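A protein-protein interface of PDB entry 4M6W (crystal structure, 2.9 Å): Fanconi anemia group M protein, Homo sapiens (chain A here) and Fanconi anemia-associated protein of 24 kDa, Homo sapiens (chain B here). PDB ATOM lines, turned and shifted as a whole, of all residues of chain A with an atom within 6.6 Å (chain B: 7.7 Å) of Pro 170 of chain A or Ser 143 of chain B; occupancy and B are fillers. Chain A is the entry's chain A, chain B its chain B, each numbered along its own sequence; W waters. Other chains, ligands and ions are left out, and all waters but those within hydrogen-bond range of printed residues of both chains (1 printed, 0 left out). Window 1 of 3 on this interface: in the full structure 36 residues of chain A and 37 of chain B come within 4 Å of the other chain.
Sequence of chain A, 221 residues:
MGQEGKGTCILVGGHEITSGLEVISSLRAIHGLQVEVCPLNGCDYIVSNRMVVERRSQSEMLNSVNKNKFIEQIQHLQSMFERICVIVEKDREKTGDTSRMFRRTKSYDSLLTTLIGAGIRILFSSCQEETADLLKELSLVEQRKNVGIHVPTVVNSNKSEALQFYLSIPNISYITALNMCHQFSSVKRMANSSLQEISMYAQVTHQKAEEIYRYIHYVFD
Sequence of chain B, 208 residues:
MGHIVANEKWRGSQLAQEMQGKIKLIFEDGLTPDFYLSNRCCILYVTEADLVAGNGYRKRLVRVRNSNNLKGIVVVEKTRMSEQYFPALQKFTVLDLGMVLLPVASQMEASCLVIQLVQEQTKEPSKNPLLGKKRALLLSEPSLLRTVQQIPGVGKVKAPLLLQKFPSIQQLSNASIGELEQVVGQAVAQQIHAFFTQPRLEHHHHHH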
ATOM      1  N   SER A  79      14.620  28.945  34.060  1.00  0.00           N
ATOM      2  CA  SER A  79      14.844  28.355  32.741  1.00  0.00           C
ATOM      3  C   SER A  79      15.141  29.404  31.651  1.00  0.00           C
ATOM      4  O   SER A  79      15.896  29.125  30.717  1.00  0.00           O
ATOM      5  CB  SER A  79      13.634  27.508  32.335  1.00  0.00           C
ATOM      6  OG  SER A  79      12.527  28.332  32.017  1.00  0.00           O
ATOM      7  N   MET A  80      14.559  30.600  31.774  1.00  0.00           N
ATOM      8  CA  MET A  80      14.658  31.631  30.727  1.00  0.00           C
ATOM      9  C   MET A  80      15.637  32.771  31.035  1.00  0.00           C
ATOM     10  O   MET A  80      16.027  33.495  30.120  1.00  0.00           O
ATOM     11  CB  MET A  80      13.297  32.284  30.448  1.00  0.00           C
ATOM     12  CG  MET A  80      12.062  31.449  30.723  1.00  0.00           C
ATOM     13  SD  MET A  80      10.594  32.447  30.417  1.00  0.00           S
ATOM     14  CE  MET A  80      10.161  31.899  28.771  1.00  0.00           C
ATOM     15  N   TYR A 166      10.199  32.405  17.219  1.00  0.00           N
ATOM     16  CA  TYR A 166      11.241  32.371  18.256  1.00  0.00           C
ATOM     17  C   TYR A 166      10.637  32.166  19.647  1.00  0.00           C
ATOM     18  O   TYR A 166      11.265  31.553  20.511  1.00  0.00           O
ATOM     19  CB  TYR A 166      12.090  33.651  18.242  1.00  0.00           C
ATOM     20  CG  TYR A 166      12.939  33.835  17.000  1.00  0.00           C
ATOM     21  CD1 TYR A 166      13.894  32.888  16.637  1.00  0.00           C
ATOM     22  CD2 TYR A 166      12.801  34.966  16.198  1.00  0.00           C
ATOM     23  CE1 TYR A 166      14.677  33.056  15.501  1.00  0.00           C
ATOM     24  CE2 TYR A 166      13.580  35.145  15.063  1.00  0.00           C
ATOM     25  CZ  TYR A 166      14.518  34.187  14.718  1.00  0.00           C
ATOM     26  OH  TYR A 166      15.296  34.360  13.594  1.00  0.00           O
ATOM     27  N   LEU A 167       9.424  32.682  19.857  1.00  0.00           N
ATOM     28  CA  LEU A 167       8.711  32.521  21.133  1.00  0.00           C
ATOM     29  C   LEU A 167       8.299  31.070  21.415  1.00  0.00           C
ATOM     30  O   LEU A 167       8.159  30.678  22.577  1.00  0.00           O
ATOM     31  CB  LEU A 167       7.468  33.422  21.186  1.00  0.00           C
ATOM     32  CG  LEU A 167       7.689  34.897  21.538  1.00  0.00           C
ATOM     33  CD1 LEU A 167       6.464  35.729  21.187  1.00  0.00           C
ATOM     34  CD2 LEU A 167       8.044  35.080  23.006  1.00  0.00           C
ATOM     35  N   SER A 168       8.110  30.281  20.359  1.00  0.00           N
ATOM     36  CA  SER A 168       7.722  28.873  20.497  1.00  0.00           C
ATOM     37  C   SER A 168       8.863  27.972  20.974  1.00  0.00           C
ATOM     38  O   SER A 168       8.633  26.818  21.323  1.00  0.00           O
ATOM     39  CB  SER A 168       7.181  28.336  19.173  1.00  0.00           C
ATOM     40  OG  SER A 168       8.213  28.240  18.210  1.00  0.00           O
ATOM     41  N   ILE A 169      10.089  28.487  20.975  1.00  0.00           N
ATOM     42  CA  ILE A 169      11.228  27.740  21.507  1.00  0.00           C
ATOM     43  C   ILE A 169      11.152  27.763  23.039  1.00  0.00           C
ATOM     44  O   ILE A 169      11.071  28.839  23.636  1.00  0.00           O
ATOM     45  CB  ILE A 169      12.583  28.324  21.041  1.00  0.00           C
ATOM     46  CG1 ILE A 169      12.637  28.438  19.501  1.00  0.00           C
ATOM     47  CG2 ILE A 169      13.730  27.455  21.553  1.00  0.00           C
ATOM     48  CD1 ILE A 169      13.874  29.130  18.954  1.00  0.00           C
ATOM     49  N   PRO A 170      11.161  26.582  23.683  1.00  0.00           N
ATOM     50  CA  PRO A 170      11.120  26.558  25.152  1.00  0.00           C
ATOM     51  C   PRO A 170      12.294  27.292  25.812  1.00  0.00           C
ATOM     52  O   PRO A 170      13.392  27.346  25.245  1.00  0.00           O
ATOM     53  CB  PRO A 170      11.162  25.058  25.482  1.00  0.00           C
ATOM     54  CG  PRO A 170      10.617  24.385  24.269  1.00  0.00           C
ATOM     55  CD  PRO A 170      11.079  25.223  23.113  1.00  0.00           C
ATOM     56  N   ASN A 171      12.034  27.850  26.997  1.00  0.00           N
ATOM     57  CA  ASN A 171      13.042  28.531  27.821  1.00  0.00           C
ATOM     58  C   ASN A 171      13.652  29.788  27.181  1.00  0.00           C
ATOM     59  O   ASN A 171      14.817  30.099  27.416  1.00  0.00           O
ATOM     60  CB  ASN A 171      14.165  27.556  28.215  1.00  0.00           C
ATOM     61  CG  ASN A 171      13.642  26.187  28.611  1.00  0.00           C
ATOM     62  OD1 ASN A 171      12.601  26.076  29.260  1.00  0.00           O
ATOM     63  ND2 ASN A 171      14.364  25.136  28.223  1.00  0.00           N
ATOM     64  N   ILE A 172      12.864  30.512  26.389  1.00  0.00           N
ATOM     65  CA  ILE A 172      13.342  31.711  25.698  1.00  0.00           C
ATOM     66  C   ILE A 172      12.550  32.925  26.167  1.00  0.00           C
ATOM     67  O   ILE A 172      11.348  33.019  25.923  1.00  0.00           O
ATOM     68  CB  ILE A 172      13.245  31.546  24.159  1.00  0.00           C
ATOM     69  CG1 ILE A 172      14.318  30.570  23.648  1.00  0.00           C
ATOM     70  CG2 ILE A 172      13.375  32.875  23.431  1.00  0.00           C
ATOM     71  CD1 ILE A 172      15.756  30.942  23.969  1.00  0.00           C
ATOM     72  N   LYS A 208      23.514  28.081  27.177  1.00  0.00           N
ATOM     73  CA  LYS A 208      22.184  28.338  26.610  1.00  0.00           C
ATOM     74  C   LYS A 208      22.220  28.273  25.086  1.00  0.00           C
ATOM     75  O   LYS A 208      21.299  27.766  24.459  1.00  0.00           O
ATOM     76  CB  LYS A 208      21.664  29.709  27.058  1.00  0.00           C
ATOM     77  CG  LYS A 208      20.153  29.865  26.977  1.00  0.00           C
ATOM     78  CD  LYS A 208      19.453  29.194  28.154  1.00  0.00           C
ATOM     79  CE  LYS A 208      17.971  28.989  27.887  1.00  0.00           C
ATOM     80  NZ  LYS A 208      17.286  30.260  27.531  1.00  0.00           N
ATOM     81  N   GLU A 211      21.960  24.728  23.963  1.00  0.00           N
ATOM     82  CA  GLU A 211      20.630  24.132  24.128  1.00  0.00           C
ATOM     83  C   GLU A 211      19.701  24.409  22.947  1.00  0.00           C
ATOM     84  O   GLU A 211      19.022  23.499  22.470  1.00  0.00           O
ATOM     85  CB  GLU A 211      19.975  24.627  25.422  1.00  0.00           C
ATOM     86  CG  GLU A 211      20.650  24.109  26.683  1.00  0.00           C
ATOM     87  CD  GLU A 211      19.961  24.554  27.960  1.00  0.00           C
ATOM     88  OE1 GLU A 211      19.045  25.406  27.893  1.00  0.00           O
ATOM     89  OE2 GLU A 211      20.347  24.050  29.036  1.00  0.00           O
ATOM     90  N   ILE A 212      19.669  25.657  22.477  1.00  0.00           N
ATOM     91  CA  ILE A 212      18.834  26.018  21.324  1.00  0.00           C
ATOM     92  C   ILE A 212      19.475  25.483  20.038  1.00  0.00           C
ATOM     93  O   ILE A 212      18.784  25.246  19.057  1.00  0.00           O
ATOM     94  CB  ILE A 212      18.519  27.544  21.223  1.00  0.00           C
ATOM     95  CG1 ILE A 212      19.569  28.315  20.415  1.00  0.00           C
ATOM     96  CG2 ILE A 212      18.328  28.181  22.599  1.00  0.00           C
ATOM     97  CD1 ILE A 212      19.176  28.565  18.971  1.00  0.00           C
ATOM     98  N   TYR A 215      18.295  22.153  19.716  1.00  0.00           N
ATOM     99  CA  TYR A 215      16.877  22.259  19.342  1.00  0.00           C
ATOM    100  C   TYR A 215      16.692  22.439  17.835  1.00  0.00           C
ATOM    101  O   TYR A 215      15.927  21.713  17.209  1.00  0.00           O
ATOM    102  CB  TYR A 215      16.222  23.420  20.095  1.00  0.00           C
ATOM    103  CG  TYR A 215      14.713  23.510  19.971  1.00  0.00           C
ATOM    104  CD1 TYR A 215      13.875  22.725  20.763  1.00  0.00           C
ATOM    105  CD2 TYR A 215      14.123  24.410  19.092  1.00  0.00           C
ATOM    106  CE1 TYR A 215      12.496  22.821  20.665  1.00  0.00           C
ATOM    107  CE2 TYR A 215      12.744  24.512  18.986  1.00  0.00           C
ATOM    108  CZ  TYR A 215      11.938  23.715  19.775  1.00  0.00           C
ATOM    109  OH  TYR A 215      10.575  23.816  19.668  1.00  0.00           O
ATOM    110  N   LEU B 138      16.899  17.569  27.746  1.00  0.00           N
ATOM    111  CA  LEU B 138      15.479  17.232  27.886  1.00  0.00           C
ATOM    112  C   LEU B 138      14.652  17.754  26.688  1.00  0.00           C
ATOM    113  O   LEU B 138      13.752  18.583  26.848  1.00  0.00           O
ATOM    114  CB  LEU B 138      14.937  17.752  29.238  1.00  0.00           C
ATOM    115  CG  LEU B 138      15.224  19.206  29.671  1.00  0.00           C
ATOM    116  CD1 LEU B 138      14.077  19.760  30.512  1.00  0.00           C
ATOM    117  CD2 LEU B 138      16.546  19.342  30.425  1.00  0.00           C
ATOM    118  N   LEU B 139      14.963  17.244  25.495  1.00  0.00           N
ATOM    119  CA  LEU B 139      14.396  17.760  24.236  1.00  0.00           C
ATOM    120  C   LEU B 139      12.972  17.244  24.026  1.00  0.00           C
ATOM    121  O   LEU B 139      12.726  16.043  24.123  1.00  0.00           O
ATOM    122  CB  LEU B 139      15.280  17.361  23.040  1.00  0.00           C
ATOM    123  CG  LEU B 139      15.568  18.390  21.932  1.00  0.00           C
ATOM    124  CD1 LEU B 139      14.295  18.995  21.357  1.00  0.00           C
ATOM    125  CD2 LEU B 139      16.505  19.490  22.417  1.00  0.00           C
ATOM    126  N   SER B 140      12.048  18.163  23.737  1.00  0.00           N
ATOM    127  CA  SER B 140      10.632  17.847  23.538  1.00  0.00           C
ATOM    128  C   SER B 140      10.212  18.003  22.068  1.00  0.00           C
ATOM    129  O   SER B 140      10.180  19.114  21.534  1.00  0.00           O
ATOM    130  CB  SER B 140       9.766  18.746  24.432  1.00  0.00           C
ATOM    131  OG  SER B 140       8.398  18.697  24.056  1.00  0.00           O
ATOM    132  N   GLU B 141       9.875  16.884  21.429  1.00  0.00           N
ATOM    133  CA  GLU B 141       9.415  16.880  20.035  1.00  0.00           C
ATOM    134  C   GLU B 141       8.069  17.599  19.837  1.00  0.00           C
ATOM    135  O   GLU B 141       7.886  18.278  18.827  1.00  0.00           O
ATOM    136  CB  GLU B 141       9.350  15.448  19.485  1.00  0.00           C
ATOM    137  CG  GLU B 141      10.699  14.736  19.444  1.00  0.00           C
ATOM    138  CD  GLU B 141      10.614  13.307  18.925  1.00  0.00           C
ATOM    139  OE1 GLU B 141       9.525  12.895  18.461  1.00  0.00           O
ATOM    140  OE2 GLU B 141      11.641  12.592  18.979  1.00  0.00           O
ATOM    141  N   PRO B 142       7.121  17.449  20.786  1.00  0.00           N
ATOM    142  CA  PRO B 142       5.880  18.231  20.694  1.00  0.00           C
ATOM    143  C   PRO B 142       6.098  19.740  20.557  1.00  0.00           C
ATOM    144  O   PRO B 142       5.368  20.392  19.817  1.00  0.00           O
ATOM    145  CB  PRO B 142       5.172  17.910  22.012  1.00  0.00           C
ATOM    146  CG  PRO B 142       5.605  16.523  22.319  1.00  0.00           C
ATOM    147  CD  PRO B 142       7.028  16.415  21.836  1.00  0.00           C
ATOM    148  N   SER B 143       7.087  20.280  21.269  1.00  0.00           N
ATOM    149  CA  SER B 143       7.462  21.692  21.134  1.00  0.00           C
ATOM    150  C   SER B 143       7.995  22.006  19.732  1.00  0.00           C
ATOM    151  O   SER B 143       7.694  23.059  19.172  1.00  0.00           O
ATOM    152  CB  SER B 143       8.498  22.090  22.193  1.00  0.00           C
ATOM    153  OG  SER B 143       7.876  22.425  23.420  1.00  0.00           O
ATOM    154  N   LEU B 144       8.783  21.090  19.170  1.00  0.00           N
ATOM    155  CA  LEU B 144       9.317  21.244  17.812  1.00  0.00           C
ATOM    156  C   LEU B 144       8.213  21.317  16.749  1.00  0.00           C
ATOM    157  O   LEU B 144       8.323  22.079  15.789  1.00  0.00           O
ATOM    158  CB  LEU B 144      10.287  20.105  17.475  1.00  0.00           C
ATOM    159  CG  LEU B 144      11.682  20.178  18.107  1.00  0.00           C
ATOM    160  CD1 LEU B 144      12.329  18.801  18.208  1.00  0.00           C
ATOM    161  CD2 LEU B 144      12.580  21.124  17.327  1.00  0.00           C
ATOM    162  N   LEU B 145       7.161  20.521  16.921  1.00  0.00           N
ATOM    163  CA  LEU B 145       6.005  20.570  16.025  1.00  0.00           C
ATOM    164  C   LEU B 145       5.244  21.888  16.183  1.00  0.00           C
ATOM    165  O   LEU B 145       4.850  22.503  15.190  1.00  0.00           O
ATOM    166  CB  LEU B 145       5.071  19.379  16.271  1.00  0.00           C
ATOM    167  CG  LEU B 145       5.563  18.009  15.781  1.00  0.00           C
ATOM    168  CD1 LEU B 145       4.757  16.885  16.410  1.00  0.00           C
ATOM    169  CD2 LEU B 145       5.500  17.911  14.264  1.00  0.00           C
ATOM    170  N   ARG B 146       5.045  22.314  17.432  1.00  0.00           N
ATOM    171  CA  ARG B 146       4.484  23.641  17.738  1.00  0.00           C
ATOM    172  C   ARG B 146       5.294  24.776  17.072  1.00  0.00           C
ATOM    173  O   ARG B 146       4.715  25.709  16.510  1.00  0.00           O
ATOM    174  CB  ARG B 146       4.395  23.865  19.262  1.00  0.00           C
ATOM    175  CG  ARG B 146       3.025  23.594  19.883  1.00  0.00           C
ATOM    176  CD  ARG B 146       2.680  22.108  19.978  1.00  0.00           C
ATOM    177  NE  ARG B 146       1.343  21.860  20.543  1.00  0.00           N
ATOM    178  CZ  ARG B 146       0.197  21.875  19.852  1.00  0.00           C
ATOM    179  NH1 ARG B 146       0.188  22.137  18.546  1.00  0.00           N
ATOM    180  NH2 ARG B 146      -0.955  21.632  20.474  1.00  0.00           N
ATOM    181  N   THR B 147       6.623  24.680  17.130  1.00  0.00           N
ATOM    182  CA  THR B 147       7.515  25.685  16.540  1.00  0.00           C
ATOM    183  C   THR B 147       7.386  25.745  15.018  1.00  0.00           C
ATOM    184  O   THR B 147       7.307  26.835  14.443  1.00  0.00           O
ATOM    185  CB  THR B 147       8.986  25.434  16.949  1.00  0.00           C
ATOM    186  OG1 THR B 147       9.142  25.707  18.347  1.00  0.00           O
ATOM    187  CG2 THR B 147       9.962  26.320  16.170  1.00  0.00           C
ATOM    188  N   VAL B 148       7.363  24.578  14.373  1.00  0.00           N
ATOM    189  CA  VAL B 148       7.181  24.507  12.919  1.00  0.00           C
ATOM    190  C   VAL B 148       5.779  24.989  12.555  1.00  0.00           C
ATOM    191  O   VAL B 148       5.611  25.703  11.565  1.00  0.00           O
ATOM    192  CB  VAL B 148       7.439  23.085  12.364  1.00  0.00           C
ATOM    193  CG1 VAL B 148       7.082  22.986  10.883  1.00  0.00           C
ATOM    194  CG2 VAL B 148       8.897  22.703  12.570  1.00  0.00           C
ATOM    195  N   GLN B 149       4.787  24.621  13.367  1.00  0.00           N
ATOM    196  CA  GLN B 149       3.402  25.100  13.188  1.00  0.00           C
ATOM    197  C   GLN B 149       3.291  26.633  13.171  1.00  0.00           C
ATOM    198  O   GLN B 149       2.288  27.173  12.707  1.00  0.00           O
ATOM    199  CB  GLN B 149       2.469  24.519  14.266  1.00  0.00           C
ATOM    200  CG  GLN B 149       1.981  23.099  13.989  1.00  0.00           C
ATOM    201  CD  GLN B 149       1.250  22.480  15.173  1.00  0.00           C
ATOM    202  OE1 GLN B 149       0.287  23.052  15.688  1.00  0.00           O
ATOM    203  NE2 GLN B 149       1.698  21.298  15.603  1.00  0.00           N
ATOM    204  N   GLN B 150       4.322  27.321  13.663  1.00  0.00           N
ATOM    205  CA  GLN B 150       4.337  28.786  13.712  1.00  0.00           C
ATOM    206  C   GLN B 150       4.796  29.414  12.388  1.00  0.00           C
ATOM    207  O   GLN B 150       4.610  30.611  12.172  1.00  0.00           O
ATOM    208  CB  GLN B 150       5.230  29.264  14.865  1.00  0.00           C
ATOM    209  CG  GLN B 150       4.579  30.306  15.761  1.00  0.00           C
ATOM    210  CD  GLN B 150       3.502  29.731  16.666  1.00  0.00           C
ATOM    211  OE1 GLN B 150       3.471  28.529  16.938  1.00  0.00           O
ATOM    212  NE2 GLN B 150       2.614  30.594  17.145  1.00  0.00           N
ATOM    213  N   ILE B 169      14.874  21.560  11.850  1.00  0.00           N
ATOM    214  CA  ILE B 169      14.573  22.959  11.500  1.00  0.00           C
ATOM    215  C   ILE B 169      15.701  23.511  10.614  1.00  0.00           C
ATOM    216  O   ILE B 169      15.459  24.332   9.724  1.00  0.00           O
ATOM    217  CB  ILE B 169      14.364  23.854  12.760  1.00  0.00           C
ATOM    218  CG1 ILE B 169      13.158  23.366  13.579  1.00  0.00           C
ATOM    219  CG2 ILE B 169      14.146  25.316  12.371  1.00  0.00           C
ATOM    220  CD1 ILE B 169      13.041  23.983  14.960  1.00  0.00           C
HETATM  221  O   HOH W   1      15.003  20.422  14.603  1.00  0.00           O
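The side-chain hydroxyl (OG) of Ser 168 of chain A sits at hydrogen-bond distance from the side-chain hydroxyl (OG1) of Thr 147 of chain B. The side-chain hydroxyl (OH) of Tyr 215 of chain A sits at hydrogen-bond distance from the backbone carbonyl oxygen (O) of Ser 143 of chain B (3.0 Å). OH of Tyr 215 of chain A sits at hydrogen-bond distance from N of Leu 144 of chain B (3.3 Å). The side-chain hydroxyl of Tyr 215 of chain A sits at hydrogen-bond distance from the side-chain hydroxyl of Thr 147 of chain B (2.7 Å).
Printed residues of chain A that touch a printed residue of chain B: Ser 168, Ile 169, Pro 170 and Tyr 215. Hydrophobic or aromatic side chains of chain A that line the printed part of chain B: Pro 170 and Tyr 215. Printed residues of chain B that touch a printed residue of chain A: Leu 139, Ser 143, Leu 144 and Thr 147. Among the printed residues, 7 pairs touch across the chains. Among the printed residues, no Asp or Glu carboxylate lies within 4 Å of a Lys or Arg side-chain nitrogen of the other chain.
The backbone NH (N) of Ser 143 of chain B sits at hydrogen-bond distance from the side-chain hydroxyl (OG) of Ser 140 of chain B, 3.5 Å away. The backbone carbonyl oxygen (O) of Ser 143 of chain B sits at hydrogen-bond distance from the side-chain hydroxyl (OG1) of Thr 147 of chain B, 3.1 Å away.
Ile 169 of chain A touches Thr 147 of chain B (N to OG1, 3.9 Å). Pro 170 of chain A touches Ser 143 of chain B (CG to OG, 3.5 Å). Tyr 215 of chain A touches Leu 139 of chain B (CD1 to CD1, 3.8 Å).
Water W1 lies within hydrogen-bond range of the backbone NH (N) of Ile 169 of chain B (3.0 Å) and the backbone carbonyl oxygen (O) of Tyr 215 of chain A (3.1 Å).
Pro 170 of chain A touches just one residue of chain B: Ser 143. Ser 143 of chain B touches just these residues of chain A: Pro 170 and Tyr 215. Of the printed residues of chain B, Ser 168 of chain A touches Thr 147 (2.7 Å). Printed residues of chain A within 4 Å of Leu 144 of chain B: Tyr 215. Of the printed residues of chain A, Leu 139 of chain B touches Tyr 215.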
